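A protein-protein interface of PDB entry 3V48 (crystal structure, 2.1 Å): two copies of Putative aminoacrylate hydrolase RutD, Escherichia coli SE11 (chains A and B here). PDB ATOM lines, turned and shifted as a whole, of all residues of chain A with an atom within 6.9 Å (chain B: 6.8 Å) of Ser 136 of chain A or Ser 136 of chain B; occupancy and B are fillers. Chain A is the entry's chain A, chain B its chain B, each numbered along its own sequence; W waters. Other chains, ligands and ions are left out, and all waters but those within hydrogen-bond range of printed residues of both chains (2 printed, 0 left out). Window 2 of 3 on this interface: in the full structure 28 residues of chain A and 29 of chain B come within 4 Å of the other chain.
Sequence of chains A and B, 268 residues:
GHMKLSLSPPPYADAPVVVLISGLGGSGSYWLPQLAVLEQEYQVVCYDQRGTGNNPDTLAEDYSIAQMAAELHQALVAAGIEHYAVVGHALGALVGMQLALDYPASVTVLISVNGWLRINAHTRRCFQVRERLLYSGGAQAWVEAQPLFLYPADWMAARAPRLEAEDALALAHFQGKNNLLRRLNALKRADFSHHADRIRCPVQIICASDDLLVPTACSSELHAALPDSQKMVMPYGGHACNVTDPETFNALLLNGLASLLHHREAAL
Among the printed residues, merely in contact across the chains: Ala 141 of chain A with Arg 132 of chain B (3.1 Å), Ser 136 of chain A with Ser 136 of chain B (3.4 Å), Arg 132 of chain A with Ala 141 of chain B (3.5 Å), Leu 133 of chain A with Leu 133 of chain B (3.8 Å), Leu 133 of chain A with Arg 132 of chain B (3.8 Å), Arg 132 of chain A with Gly 137 of chain B (3.8 Å) and Arg 132 of chain A with Leu 133 of chain B (3.8 Å).
Leu 134 of chain A touches none of the printed residues of chain B.
Printed residues of chain B within 4 Å of Ser 136 of chain A: Ser 136 (3.4 Å).
Of the printed residues of chain A, Ser 136 of chain B touches Ser 136.
Of the printed residues of chain A, Gly 137 of chain B touches Arg 132 (3.8 Å).
Of the printed residues of chain A, Ala 141 of chain B touches Arg 132 (3.5 Å).
The nearest printed residue of chain A that does not touch Ser 136 of chain B is Arg 132 of chain A (4.7 Å).
The nearest printed residue of chain A that does not touch Gly 137 of chain B is Ser 136 of chain A (6.3 Å).
Arg 132 of chain A touches Leu 133 of chain B, and with the chains exchanged Leu 133 of chain A touches Arg 132 of chain B.
Arg 132 of chain A touches Ala 141 of chain B, and with the chains exchanged Ala 141 of chain A touches Arg 132 of chain B.
Leu 133 of chain B touches its own counterpart, Leu 133 of chain A.
Ser 136 of chain A touches its own counterpart, Ser 136 of chain B.
9 positions are printed for both chains.
Of the 7 pairs that touch across the chains among the printed residues, 6 have their exchanged pair printed and touching as well.
Water W1 lies within hydrogen-bond range of the side-chain hydroxyl (OG) of Ser 136 of chain B (2.5 Å), the backbone NH (N) of Gly 137 of chain B (3.3 Å) and the guanidinium group (NH1) of Arg 132 of chain A (3.4 Å).
Water W2 lies within hydrogen-bond range of the guanidinium group (NH2) of Arg 132 of chain B (2.9 Å) and the backbone NH (N) of Ala 141 of chain A (3.3 Å).
The backbone carbonyl oxygen (O) of Arg 132 of chain A is in hydrogen-bond range of the side-chain hydroxyl (OG) of Ser 136 of chain A.
The backbone carbonyl oxygen of Leu 133 of chain A sits at hydrogen-bond distance from the side-chain hydroxyl of Ser 136 of chain A (3.5 Å).
N of Gly 138 of chain A lies within hydrogen-bond range of O of Leu 133 of chain A (3.4 Å).
The side-chain hydroxyl (OG) of Ser 136 of chain B sits at hydrogen-bond distance from the backbone carbonyl oxygen (O) of Arg 132 of chain B (2.8 Å).
The backbone carbonyl oxygen of Leu 133 of chain B lies within hydrogen-bond range of the backbone NH of Gly 138 of chain B, at 3.4 Å.
Of the 9 printed residues of chain B, 5 touch a printed residue of chain A.
Hydrophobic or aromatic side chains of chain B within 4 Å of the printed part of chain A: Leu 133 and Ala 141.
Among the printed residues, 7 pairs touch across the chains.
Among the printed residues, no Asp or Glu carboxylate lies within 4 Å of a Lys or Arg side-chain nitrogen of the other chain.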
ATOM      1  N   GLU A 131      20.541  15.876 -10.214  1.00  0.00           N
ATOM      2  CA  GLU A 131      19.572  14.803 -10.017  1.00  0.00           C
ATOM      3  C   GLU A 131      20.101  13.504 -10.594  1.00  0.00           C
ATOM      4  O   GLU A 131      20.072  12.468  -9.928  1.00  0.00           O
ATOM      5  CB  GLU A 131      18.222  15.127 -10.636  1.00  0.00           C
ATOM      6  CG  GLU A 131      17.343  16.062  -9.817  1.00  0.00           C
ATOM      7  CD  GLU A 131      16.333  16.831 -10.686  1.00  0.00           C
ATOM      8  OE1 GLU A 131      15.943  16.316 -11.777  1.00  0.00           O
ATOM      9  OE2 GLU A 131      15.931  17.957 -10.271  1.00  0.00           O
ATOM     10  N   ARG A 132      20.653  13.588 -11.809  1.00  0.00           N
ATOM     11  CA  ARG A 132      21.242  12.407 -12.432  1.00  0.00           C
ATOM     12  C   ARG A 132      22.278  11.776 -11.511  1.00  0.00           C
ATOM     13  O   ARG A 132      22.341  10.583 -11.383  1.00  0.00           O
ATOM     14  CB  ARG A 132      21.944  12.732 -13.746  1.00  0.00           C
ATOM     15  CG  ARG A 132      21.050  12.847 -14.936  1.00  0.00           C
ATOM     16  CD  ARG A 132      21.938  13.212 -16.108  1.00  0.00           C
ATOM     17  NE  ARG A 132      21.186  13.470 -17.316  1.00  0.00           N
ATOM     18  CZ  ARG A 132      20.603  12.516 -18.033  1.00  0.00           C
ATOM     19  NH1 ARG A 132      20.637  11.227 -17.627  1.00  0.00           N
ATOM     20  NH2 ARG A 132      19.940  12.841 -19.124  1.00  0.00           N
ATOM     21  N   LEU A 133      23.117  12.615 -10.908  1.00  0.00           N
ATOM     22  CA  LEU A 133      24.159  12.122 -10.028  1.00  0.00           C
ATOM     23  C   LEU A 133      23.529  11.453  -8.810  1.00  0.00           C
ATOM     24  O   LEU A 133      23.947  10.357  -8.396  1.00  0.00           O
ATOM     25  CB  LEU A 133      25.067  13.253  -9.604  1.00  0.00           C
ATOM     26  CG  LEU A 133      25.892  13.879 -10.722  1.00  0.00           C
ATOM     27  CD1 LEU A 133      26.596  15.122 -10.208  1.00  0.00           C
ATOM     28  CD2 LEU A 133      26.840  12.847 -11.314  1.00  0.00           C
ATOM     29  N   LEU A 134      22.524  12.117  -8.239  1.00  0.00           N
ATOM     30  CA  LEU A 134      21.800  11.551  -7.097  1.00  0.00           C
ATOM     31  C   LEU A 134      21.283  10.156  -7.408  1.00  0.00           C
ATOM     32  O   LEU A 134      21.603   9.200  -6.684  1.00  0.00           O
ATOM     33  CB  LEU A 134      20.621  12.434  -6.675  1.00  0.00           C
ATOM     34  CG  LEU A 134      19.894  12.015  -5.403  1.00  0.00           C
ATOM     35  CD1 LEU A 134      20.862  11.900  -4.223  1.00  0.00           C
ATOM     36  CD2 LEU A 134      18.788  12.997  -5.093  1.00  0.00           C
ATOM     37  N   TYR A 135      20.507  10.046  -8.487  1.00  0.00           N
ATOM     38  CA  TYR A 135      19.854   8.793  -8.864  1.00  0.00           C
ATOM     39  C   TYR A 135      20.810   7.692  -9.219  1.00  0.00           C
ATOM     40  O   TYR A 135      20.519   6.542  -8.932  1.00  0.00           O
ATOM     41  CB  TYR A 135      18.901   8.965 -10.050  1.00  0.00           C
ATOM     42  CG  TYR A 135      17.774   9.898  -9.783  1.00  0.00           C
ATOM     43  CD1 TYR A 135      16.992   9.782  -8.651  1.00  0.00           C
ATOM     44  CD2 TYR A 135      17.481  10.889 -10.656  1.00  0.00           C
ATOM     45  CE1 TYR A 135      15.939  10.655  -8.410  1.00  0.00           C
ATOM     46  CE2 TYR A 135      16.446  11.774 -10.416  1.00  0.00           C
ATOM     47  CZ  TYR A 135      15.671  11.641  -9.304  1.00  0.00           C
ATOM     48  OH  TYR A 135      14.657  12.535  -9.131  1.00  0.00           O
ATOM     49  N   SER A 136      21.938   8.030  -9.831  1.00  0.00           N
ATOM     50  CA  SER A 136      22.894   7.046 -10.336  1.00  0.00           C
ATOM     51  C   SER A 136      24.023   6.726  -9.368  1.00  0.00           C
ATOM     52  O   SER A 136      24.603   5.635  -9.416  1.00  0.00           O
ATOM     53  CB  SER A 136      23.529   7.546 -11.643  1.00  0.00           C
ATOM     54  OG  SER A 136      24.408   8.641 -11.406  1.00  0.00           O
ATOM     55  N   GLY A 137      24.365   7.683  -8.525  1.00  0.00           N
ATOM     56  CA  GLY A 137      25.527   7.517  -7.627  1.00  0.00           C
ATOM     57  C   GLY A 137      25.303   7.854  -6.177  1.00  0.00           C
ATOM     58  O   GLY A 137      26.263   7.894  -5.390  1.00  0.00           O
ATOM     59  N   GLY A 138      24.060   8.173  -5.834  1.00  0.00           N
ATOM     60  CA  GLY A 138      23.707   8.443  -4.466  1.00  0.00           C
ATOM     61  C   GLY A 138      24.335   9.707  -3.888  1.00  0.00           C
ATOM     62  O   GLY A 138      24.763  10.636  -4.585  1.00  0.00           O
ATOM     63  N   ALA A 141      27.886  10.814  -4.911  1.00  0.00           N
ATOM     64  CA  ALA A 141      28.058  11.490  -6.201  1.00  0.00           C
ATOM     65  C   ALA A 141      27.456  12.912  -6.133  1.00  0.00           C
ATOM     66  O   ALA A 141      28.014  13.851  -6.649  1.00  0.00           O
ATOM     67  CB  ALA A 141      27.409  10.686  -7.282  1.00  0.00           C
ATOM     68  N   GLU B 131      32.521  11.907 -15.867  1.00  0.00           N
ATOM     69  CA  GLU B 131      32.578  10.443 -16.160  1.00  0.00           C
ATOM     70  C   GLU B 131      31.353   9.738 -15.614  1.00  0.00           C
ATOM     71  O   GLU B 131      30.726   8.931 -16.299  1.00  0.00           O
ATOM     72  CB  GLU B 131      33.863   9.797 -15.645  1.00  0.00           C
ATOM     73  CG  GLU B 131      35.058  10.086 -16.557  1.00  0.00           C
ATOM     74  CD  GLU B 131      36.448   9.885 -15.904  1.00  0.00           C
ATOM     75  OE1 GLU B 131      36.670   8.897 -15.176  1.00  0.00           O
ATOM     76  OE2 GLU B 131      37.343  10.709 -16.165  1.00  0.00           O
ATOM     77  N   ARG B 132      30.998  10.058 -14.376  1.00  0.00           N
ATOM     78  CA  ARG B 132      29.805   9.494 -13.742  1.00  0.00           C
ATOM     79  C   ARG B 132      28.577   9.739 -14.626  1.00  0.00           C
ATOM     80  O   ARG B 132      27.732   8.857 -14.809  1.00  0.00           O
ATOM     81  CB  ARG B 132      29.608  10.074 -12.328  1.00  0.00           C
ATOM     82  CG  ARG B 132      28.525   9.372 -11.525  1.00  0.00           C
ATOM     83  CD  ARG B 132      28.538   9.701 -10.033  1.00  0.00           C
ATOM     84  NE  ARG B 132      29.745   9.272  -9.328  1.00  0.00           N
ATOM     85  CZ  ARG B 132      30.015   8.014  -8.963  1.00  0.00           C
ATOM     86  NH1 ARG B 132      29.159   7.026  -9.245  1.00  0.00           N
ATOM     87  NH2 ARG B 132      31.142   7.752  -8.295  1.00  0.00           N
ATOM     88  N   LEU B 133      28.477  10.950 -15.184  1.00  0.00           N
ATOM     89  CA  LEU B 133      27.356  11.267 -16.072  1.00  0.00           C
ATOM     90  C   LEU B 133      27.440  10.429 -17.335  1.00  0.00           C
ATOM     91  O   LEU B 133      26.431   9.900 -17.809  1.00  0.00           O
ATOM     92  CB  LEU B 133      27.347  12.737 -16.439  1.00  0.00           C
ATOM     93  CG  LEU B 133      27.030  13.635 -15.248  1.00  0.00           C
ATOM     94  CD1 LEU B 133      27.249  15.101 -15.605  1.00  0.00           C
ATOM     95  CD2 LEU B 133      25.587  13.325 -14.826  1.00  0.00           C
ATOM     96  N   LEU B 134      28.638  10.354 -17.898  1.00  0.00           N
ATOM     97  CA  LEU B 134      28.878   9.473 -19.058  1.00  0.00           C
ATOM     98  C   LEU B 134      28.365   8.047 -18.805  1.00  0.00           C
ATOM     99  O   LEU B 134      27.539   7.540 -19.572  1.00  0.00           O
ATOM    100  CB  LEU B 134      30.355   9.438 -19.449  1.00  0.00           C
ATOM    101  CG  LEU B 134      30.676   8.712 -20.748  1.00  0.00           C
ATOM    102  CD1 LEU B 134      29.873   9.348 -21.850  1.00  0.00           C
ATOM    103  CD2 LEU B 134      32.175   8.745 -21.030  1.00  0.00           C
ATOM    104  N   TYR B 135      28.837   7.425 -17.718  1.00  0.00           N
ATOM    105  CA  TYR B 135      28.519   6.017 -17.431  1.00  0.00           C
ATOM    106  C   TYR B 135      27.048   5.781 -17.127  1.00  0.00           C
ATOM    107  O   TYR B 135      26.501   4.747 -17.478  1.00  0.00           O
ATOM    108  CB  TYR B 135      29.355   5.478 -16.280  1.00  0.00           C
ATOM    109  CG  TYR B 135      30.836   5.534 -16.540  1.00  0.00           C
ATOM    110  CD1 TYR B 135      31.379   5.035 -17.719  1.00  0.00           C
ATOM    111  CD2 TYR B 135      31.690   6.122 -15.622  1.00  0.00           C
ATOM    112  CE1 TYR B 135      32.731   5.116 -17.977  1.00  0.00           C
ATOM    113  CE2 TYR B 135      33.030   6.208 -15.875  1.00  0.00           C
ATOM    114  CZ  TYR B 135      33.536   5.716 -17.049  1.00  0.00           C
ATOM    115  OH  TYR B 135      34.868   5.788 -17.256  1.00  0.00           O
ATOM    116  N   SER B 136      26.408   6.768 -16.518  1.00  0.00           N
ATOM    117  CA  SER B 136      25.022   6.613 -16.080  1.00  0.00           C
ATOM    118  C   SER B 136      23.991   7.167 -17.057  1.00  0.00           C
ATOM    119  O   SER B 136      22.851   6.680 -17.099  1.00  0.00           O
ATOM    120  CB  SER B 136      24.844   7.295 -14.733  1.00  0.00           C
ATOM    121  OG  SER B 136      24.913   8.694 -14.874  1.00  0.00           O
ATOM    122  N   GLY B 137      24.378   8.185 -17.806  1.00  0.00           N
ATOM    123  CA  GLY B 137      23.464   8.873 -18.710  1.00  0.00           C
ATOM    124  C   GLY B 137      23.944   9.049 -20.160  1.00  0.00           C
ATOM    125  O   GLY B 137      23.283   9.708 -20.947  1.00  0.00           O
ATOM    126  N   GLY B 138      25.069   8.438 -20.502  1.00  0.00           N
ATOM    127  CA  GLY B 138      25.569   8.420 -21.862  1.00  0.00           C
ATOM    128  C   GLY B 138      25.973   9.781 -22.409  1.00  0.00           C
ATOM    129  O   GLY B 138      26.228  10.746 -21.663  1.00  0.00           O
ATOM    130  N   ALA B 141      23.808  12.808 -21.265  1.00  0.00           N
ATOM    131  CA  ALA B 141      24.067  13.368 -19.933  1.00  0.00           C
ATOM    132  C   ALA B 141      25.399  14.105 -19.976  1.00  0.00           C
ATOM    133  O   ALA B 141      25.548  15.148 -19.373  1.00  0.00           O
ATOM    134  CB  ALA B 141      24.062  12.297 -18.865  1.00  0.00           C
HETATM  135  O   HOH W   1      22.909   9.962 -15.492  1.00  0.00           O
HETATM  136  O   HOH W   2      30.493   9.026  -5.784  1.00  0.00           O
